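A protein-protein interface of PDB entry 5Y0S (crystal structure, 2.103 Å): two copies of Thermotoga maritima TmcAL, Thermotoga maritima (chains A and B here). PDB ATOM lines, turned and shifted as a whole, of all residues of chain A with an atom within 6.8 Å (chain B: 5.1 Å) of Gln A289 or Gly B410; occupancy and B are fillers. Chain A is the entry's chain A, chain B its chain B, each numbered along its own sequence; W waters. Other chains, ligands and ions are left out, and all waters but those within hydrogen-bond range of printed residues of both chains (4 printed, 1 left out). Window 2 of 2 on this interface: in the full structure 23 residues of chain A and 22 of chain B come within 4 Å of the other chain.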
ATOM      1  N   LEU A 258      33.881  14.779  10.658  1.00  0.00           N
ATOM      2  CA  LEU A 258      33.163  15.113  11.864  1.00  0.00           C
ATOM      3  C   LEU A 258      33.898  14.546  13.095  1.00  0.00           C
ATOM      4  O   LEU A 258      34.040  15.231  14.101  1.00  0.00           O
ATOM      5  CB  LEU A 258      31.722  14.610  11.776  1.00  0.00           C
ATOM      6  CG  LEU A 258      30.835  14.863  12.997  1.00  0.00           C
ATOM      7  CD1 LEU A 258      30.832  16.333  13.333  1.00  0.00           C
ATOM      8  CD2 LEU A 258      29.413  14.361  12.763  1.00  0.00           C
ATOM      9  N   ARG A 262      35.894  16.638  16.286  1.00  0.00           N
ATOM     10  CA  ARG A 262      35.723  16.327  17.709  1.00  0.00           C
ATOM     11  C   ARG A 262      37.032  16.155  18.457  1.00  0.00           C
ATOM     12  O   ARG A 262      37.046  16.099  19.682  1.00  0.00           O
ATOM     13  CB  ARG A 262      34.904  15.060  17.900  1.00  0.00           C
ATOM     14  CG  ARG A 262      33.482  15.222  17.510  1.00  0.00           C
ATOM     15  CD  ARG A 262      32.657  14.092  18.033  1.00  0.00           C
ATOM     16  NE  ARG A 262      31.272  14.318  17.667  1.00  0.00           N
ATOM     17  CZ  ARG A 262      30.267  13.558  18.064  1.00  0.00           C
ATOM     18  NH1 ARG A 262      30.498  12.519  18.854  1.00  0.00           N
ATOM     19  NH2 ARG A 262      29.033  13.855  17.679  1.00  0.00           N
ATOM     20  N   HIS A 284      33.486  24.049  16.548  1.00  0.00           N
ATOM     21  CA  HIS A 284      33.721  23.332  17.793  1.00  0.00           C
ATOM     22  C   HIS A 284      32.420  22.776  18.381  1.00  0.00           C
ATOM     23  O   HIS A 284      32.338  21.593  18.717  1.00  0.00           O
ATOM     24  CB  HIS A 284      34.415  24.245  18.804  1.00  0.00           C
ATOM     25  CG  HIS A 284      34.815  23.545  20.065  1.00  0.00           C
ATOM     26  ND1 HIS A 284      34.005  23.499  21.178  1.00  0.00           N
ATOM     27  CD2 HIS A 284      35.927  22.836  20.379  1.00  0.00           C
ATOM     28  CE1 HIS A 284      34.609  22.808  22.130  1.00  0.00           C
ATOM     29  NE2 HIS A 284      35.776  22.396  21.670  1.00  0.00           N
ATOM     30  N   VAL A 285      31.407  23.632  18.490  1.00  0.00           N
ATOM     31  CA  VAL A 285      30.127  23.251  19.082  1.00  0.00           C
ATOM     32  C   VAL A 285      29.332  22.292  18.197  1.00  0.00           C
ATOM     33  O   VAL A 285      28.816  21.289  18.687  1.00  0.00           O
ATOM     34  CB  VAL A 285      29.254  24.485  19.378  1.00  0.00           C
ATOM     35  CG1 VAL A 285      27.895  24.061  19.919  1.00  0.00           C
ATOM     36  CG2 VAL A 285      29.954  25.421  20.356  1.00  0.00           C
ATOM     37  N   CYS A 286      29.229  22.598  16.903  1.00  0.00           N
ATOM     38  CA  CYS A 286      28.464  21.743  15.986  1.00  0.00           C
ATOM     39  C   CYS A 286      29.049  20.350  15.822  1.00  0.00           C
ATOM     40  O   CYS A 286      28.312  19.382  15.622  1.00  0.00           O
ATOM     41  CB  CYS A 286      28.346  22.386  14.605  1.00  0.00           C
ATOM     42  SG  CYS A 286      27.177  23.758  14.538  1.00  0.00           S
ATOM     43  N   ALA A 287      30.370  20.241  15.879  1.00  0.00           N
ATOM     44  CA  ALA A 287      31.004  18.939  15.723  1.00  0.00           C
ATOM     45  C   ALA A 287      30.654  18.029  16.899  1.00  0.00           C
ATOM     46  O   ALA A 287      30.589  16.806  16.766  1.00  0.00           O
ATOM     47  CB  ALA A 287      32.508  19.087  15.595  1.00  0.00           C
ATOM     48  N   ARG A 288      30.446  18.643  18.055  1.00  0.00           N
ATOM     49  CA  ARG A 288      30.072  17.918  19.251  1.00  0.00           C
ATOM     50  C   ARG A 288      28.571  17.630  19.304  1.00  0.00           C
ATOM     51  O   ARG A 288      28.163  16.632  19.882  1.00  0.00           O
ATOM     52  CB  ARG A 288      30.540  18.688  20.500  1.00  0.00           C
ATOM     53  CG  ARG A 288      32.014  18.404  20.838  1.00  0.00           C
ATOM     54  CD  ARG A 288      32.751  19.622  21.388  1.00  0.00           C
ATOM     55  NE  ARG A 288      34.194  19.382  21.485  1.00  0.00           N
ATOM     56  CZ  ARG A 288      35.050  19.534  20.474  1.00  0.00           C
ATOM     57  NH1 ARG A 288      34.617  19.920  19.278  1.00  0.00           N
ATOM     58  NH2 ARG A 288      36.345  19.297  20.649  1.00  0.00           N
ATOM     59  N   GLN A 289      27.753  18.504  18.718  1.00  0.00           N
ATOM     60  CA  GLN A 289      26.296  18.371  18.835  1.00  0.00           C
ATOM     61  C   GLN A 289      25.568  17.708  17.648  1.00  0.00           C
ATOM     62  O   GLN A 289      24.372  17.452  17.725  1.00  0.00           O
ATOM     63  CB  GLN A 289      25.686  19.747  19.084  1.00  0.00           C
ATOM     64  CG  GLN A 289      26.108  20.369  20.411  1.00  0.00           C
ATOM     65  CD  GLN A 289      25.772  19.496  21.624  1.00  0.00           C
ATOM     66  OE1 GLN A 289      24.677  18.930  21.724  1.00  0.00           O
ATOM     67  NE2 GLN A 289      26.720  19.392  22.556  1.00  0.00           N
ATOM     68  N   THR A 290      26.282  17.402  16.572  1.00  0.00           N
ATOM     69  CA  THR A 290      25.677  16.717  15.432  1.00  0.00           C
ATOM     70  C   THR A 290      26.292  15.328  15.269  1.00  0.00           C
ATOM     71  O   THR A 290      27.397  15.080  15.757  1.00  0.00           O
ATOM     72  CB  THR A 290      25.854  17.504  14.127  1.00  0.00           C
ATOM     73  OG1 THR A 290      27.245  17.757  13.906  1.00  0.00           O
ATOM     74  CG2 THR A 290      25.103  18.829  14.203  1.00  0.00           C
ATOM     75  N   GLY A 291      25.553  14.420  14.627  1.00  0.00           N
ATOM     76  CA  GLY A 291      25.996  13.044  14.434  1.00  0.00           C
ATOM     77  C   GLY A 291      26.372  12.639  13.016  1.00  0.00           C
ATOM     78  O   GLY A 291      26.810  11.503  12.779  1.00  0.00           O
ATOM     79  N   ASP A 295      24.409  16.984   8.882  1.00  0.00           N
ATOM     80  CA  ASP A 295      23.839  17.736   9.991  1.00  0.00           C
ATOM     81  C   ASP A 295      24.815  18.796  10.492  1.00  0.00           C
ATOM     82  O   ASP A 295      24.411  19.903  10.828  1.00  0.00           O
ATOM     83  CB  ASP A 295      23.434  16.800  11.126  1.00  0.00           C
ATOM     84  CG  ASP A 295      22.206  15.977  10.788  1.00  0.00           C
ATOM     85  OD1 ASP A 295      21.483  16.354   9.843  1.00  0.00           O
ATOM     86  OD2 ASP A 295      21.960  14.959  11.465  1.00  0.00           O
ATOM     87  N   CYS A 299      24.199  22.832  10.754  1.00  0.00           N
ATOM     88  CA  CYS A 299      24.371  23.502  12.044  1.00  0.00           C
ATOM     89  C   CYS A 299      25.292  24.719  11.909  1.00  0.00           C
ATOM     90  O   CYS A 299      24.989  25.787  12.423  1.00  0.00           O
ATOM     91  CB  CYS A 299      24.925  22.516  13.089  1.00  0.00           C
ATOM     92  SG  CYS A 299      25.207  23.201  14.756  1.00  0.00           S
ATOM     93  N   ASN B 396      33.863  11.551  23.323  1.00  0.00           N
ATOM     94  CA  ASN B 396      33.252  12.148  22.136  1.00  0.00           C
ATOM     95  C   ASN B 396      33.682  11.447  20.833  1.00  0.00           C
ATOM     96  O   ASN B 396      32.871  11.246  19.924  1.00  0.00           O
ATOM     97  CB  ASN B 396      33.579  13.640  22.081  1.00  0.00           C
ATOM     98  CG  ASN B 396      32.836  14.431  23.159  1.00  0.00           C
ATOM     99  OD1 ASN B 396      31.904  13.914  23.784  1.00  0.00           O
ATOM    100  ND2 ASN B 396      33.238  15.680  23.371  1.00  0.00           N
ATOM    101  N   SER B 399      31.964   7.993  20.701  1.00  0.00           N
ATOM    102  CA  SER B 399      30.542   8.080  20.378  1.00  0.00           C
ATOM    103  C   SER B 399      30.250   8.089  18.883  1.00  0.00           C
ATOM    104  O   SER B 399      29.148   7.728  18.467  1.00  0.00           O
ATOM    105  CB  SER B 399      29.921   9.334  21.013  1.00  0.00           C
ATOM    106  OG  SER B 399      29.705   9.128  22.393  1.00  0.00           O
ATOM    107  N   ARG B 408      24.900   9.358  18.115  1.00  0.00           N
ATOM    108  CA  ARG B 408      26.244   9.944  17.976  1.00  0.00           C
ATOM    109  C   ARG B 408      26.381  11.424  18.363  1.00  0.00           C
ATOM    110  O   ARG B 408      27.497  11.949  18.413  1.00  0.00           O
ATOM    111  CB  ARG B 408      26.731   9.773  16.532  1.00  0.00           C
ATOM    112  CG  ARG B 408      26.788   8.331  16.088  1.00  0.00           C
ATOM    113  CD  ARG B 408      27.192   8.183  14.619  1.00  0.00           C
ATOM    114  NE  ARG B 408      27.406   6.769  14.341  1.00  0.00           N
ATOM    115  CZ  ARG B 408      27.680   6.257  13.151  1.00  0.00           C
ATOM    116  NH1 ARG B 408      27.767   7.037  12.080  1.00  0.00           N
ATOM    117  NH2 ARG B 408      27.859   4.952  13.043  1.00  0.00           N
ATOM    118  N   CME B 409      25.255  12.082  18.624  1.00  0.00           N
ATOM    119  CA  CME B 409      25.219  13.488  19.007  1.00  0.00           C
ATOM    120  CB  CME B 409      23.866  14.178  18.799  1.00  0.00           C
ATOM    121  SG  CME B 409      23.361  14.209  17.140  1.00  0.00           S
ATOM    122  SD  CME B 409      22.370  12.411  16.711  1.00  0.00           S
ATOM    123  CE  CME B 409      20.824  12.908  16.028  1.00  0.00           C
ATOM    124  CZ  CME B 409      19.612  12.299  16.708  1.00  0.00           C
ATOM    125  OH  CME B 409      19.682  12.634  18.088  1.00  0.00           O
ATOM    126  C   CME B 409      25.359  13.712  20.503  1.00  0.00           C
ATOM    127  O   CME B 409      24.899  12.956  21.357  1.00  0.00           O
ATOM    128  N   GLY B 410      25.989  14.838  20.822  1.00  0.00           N
ATOM    129  CA  GLY B 410      26.065  15.324  22.188  1.00  0.00           C
ATOM    130  C   GLY B 410      27.301  14.825  22.912  1.00  0.00           C
ATOM    131  O   GLY B 410      27.959  13.893  22.465  1.00  0.00           O
ATOM    132  N   GLU B 411      27.617  15.450  24.039  1.00  0.00           N
ATOM    133  CA  GLU B 411      28.764  15.043  24.823  1.00  0.00           C
ATOM    134  C   GLU B 411      28.292  14.253  26.030  1.00  0.00           C
ATOM    135  O   GLU B 411      27.756  14.817  26.984  1.00  0.00           O
ATOM    136  CB  GLU B 411      29.580  16.258  25.263  1.00  0.00           C
ATOM    137  CG  GLU B 411      30.064  17.123  24.106  1.00  0.00           C
ATOM    138  CD  GLU B 411      31.018  18.219  24.553  1.00  0.00           C
ATOM    139  OE1 GLU B 411      30.554  19.363  24.723  1.00  0.00           O
ATOM    140  OE2 GLU B 411      32.228  17.939  24.741  1.00  0.00           O
ATOM    141  N   ARG B 412      28.530  12.948  25.997  1.00  0.00           N
ATOM    142  CA  ARG B 412      27.994  12.062  27.015  1.00  0.00           C
ATOM    143  C   ARG B 412      28.572  12.346  28.383  1.00  0.00           C
ATOM    144  O   ARG B 412      27.943  12.014  29.379  1.00  0.00           O
ATOM    145  CB  ARG B 412      28.242  10.596  26.669  1.00  0.00           C
ATOM    146  CG  ARG B 412      27.624  10.161  25.359  1.00  0.00           C
ATOM    147  CD  ARG B 412      27.467   8.657  25.315  1.00  0.00           C
ATOM    148  NE  ARG B 412      26.053   8.322  25.321  1.00  0.00           N
ATOM    149  CZ  ARG B 412      25.510   7.376  26.069  1.00  0.00           C
ATOM    150  NH1 ARG B 412      26.265   6.660  26.892  1.00  0.00           N
ATOM    151  NH2 ARG B 412      24.205   7.164  26.002  1.00  0.00           N
HETATM  152  O   HOH W   1      27.265   9.441  11.030  1.00  0.00           O
HETATM  153  O   HOH W   2      35.822  16.378  22.106  1.00  0.00           O
HETATM  154  O   HOH W   3      26.198  17.540  25.043  1.00  0.00           O
HETATM  155  O   HOH W   4      22.928  14.751  13.924  1.00  0.00           O
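O of Gln A289 lies close to SG of CME B409, at 3.4 Å.
NH2 of Arg A262 lies within hydrogen-bond range of O of Arg B408 (2.6 Å).
The backbone carbonyl oxygen (O) of Arg A288 is in hydrogen-bond range of the backbone NH (N) of Gly B410.
The backbone NH (N) of Gly A291 lies within hydrogen-bond range of SG of CME B409 (3.3 Å).
The guanidinium group (NH1) of Arg A262 is in hydrogen-bond range of the backbone carbonyl oxygen (O) of Asn B396 (2.9 Å).
The backbone carbonyl oxygen of Cys A286 is in hydrogen-bond range of the side-chain hydroxyl of Thr A290 (2.6 Å).
The guanidinium group (NE) of Arg A262 is in hydrogen-bond range of the backbone carbonyl oxygen (O) of Ala A287 (2.7 Å).
O of Arg A262 sits at hydrogen-bond distance from NH2 of Arg A288.
The backbone carbonyl oxygen of His A284 sits at hydrogen-bond distance from the guanidinium group of Arg A288.
SG of Cys A299 forms a disulfide with SG of Cys A286, at 2.1 Å.
The guanidinium group (NH2) of Arg A262 is in hydrogen-bond range of the backbone carbonyl oxygen (O) of Thr A290.
Among the printed residues, merely in contact across the chains: Thr A290 with CME B409 (3.7 Å), Arg A288 with Glu B411 (3.8 Å), Gly A291 with Arg B408 (3.8 Å), Arg A262 with Ser B399 (3.9 Å), Gln A289 with Gly B410 (3.9 Å) and Arg A288 with Asn B396 (3.9 Å).
Of the printed residues of chain B, Arg A262 touches Asn B396, Ser B399 and Arg B408.
Cys A286 touches none of the printed residues of chain B.
Ala A287 touches none of the printed residues of chain B.
Of chain B, only CME B409 (3.4 Å) and Gly B410 (3.9 Å) come within 4 Å of Gln A289.
Printed residues of chain B within 4 Å of Thr A290: CME B409 (3.7 Å).
Of the printed residues of chain B, Gly A291 touches Arg B408 and CME B409.
Of the printed residues of chain A, Asn B396 touches Arg A262 (2.9 Å) and Arg A288 (3.9 Å).
Of the printed residues of chain A, Ser B399 touches Arg A262.
Of chain A, only Arg A288 (3.0 Å) and Gln A289 (3.9 Å) come within 4 Å of Gly B410.
The nearest printed residue of chain A that does not touch Ser B399 is Gly A291 (7.2 Å).
Of the 12 printed residues of chain A, 5 touch a printed residue of chain B.
Printed residues of chain A that touch a printed residue of chain B: Arg A262, Arg A288, Gln A289, Thr A290 and Gly A291.
Among the printed residues, 11 pairs touch across the chains.
Among the printed residues, no Asp or Glu carboxylate lies within 4 Å of a Lys or Arg side-chain nitrogen of the other chain.
No position is printed for both chains.
Of the 11 pairs that touch across the chains among the printed residues, none has its exchanged pair printed and touching as well.
Water W4 lies within hydrogen-bond range of OD2 of Asp A295, N of Gly A291 and SG of CME B409.
Water W1 lies within hydrogen-bond range of the guanidinium group (NH1) of Arg B408 and the backbone carbonyl oxygen (O) of Gly A291.
Water W3 lies within hydrogen-bond range of N of Glu B411 (2.7 Å) and NE2 of Gln A289 (3.1 Å).
Water W2 lies within hydrogen-bond range of O of Arg A262 (2.7 Å), ND2 of Asn B396 (3.0 Å) and NH2 of Arg A288 (3.3 Å).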
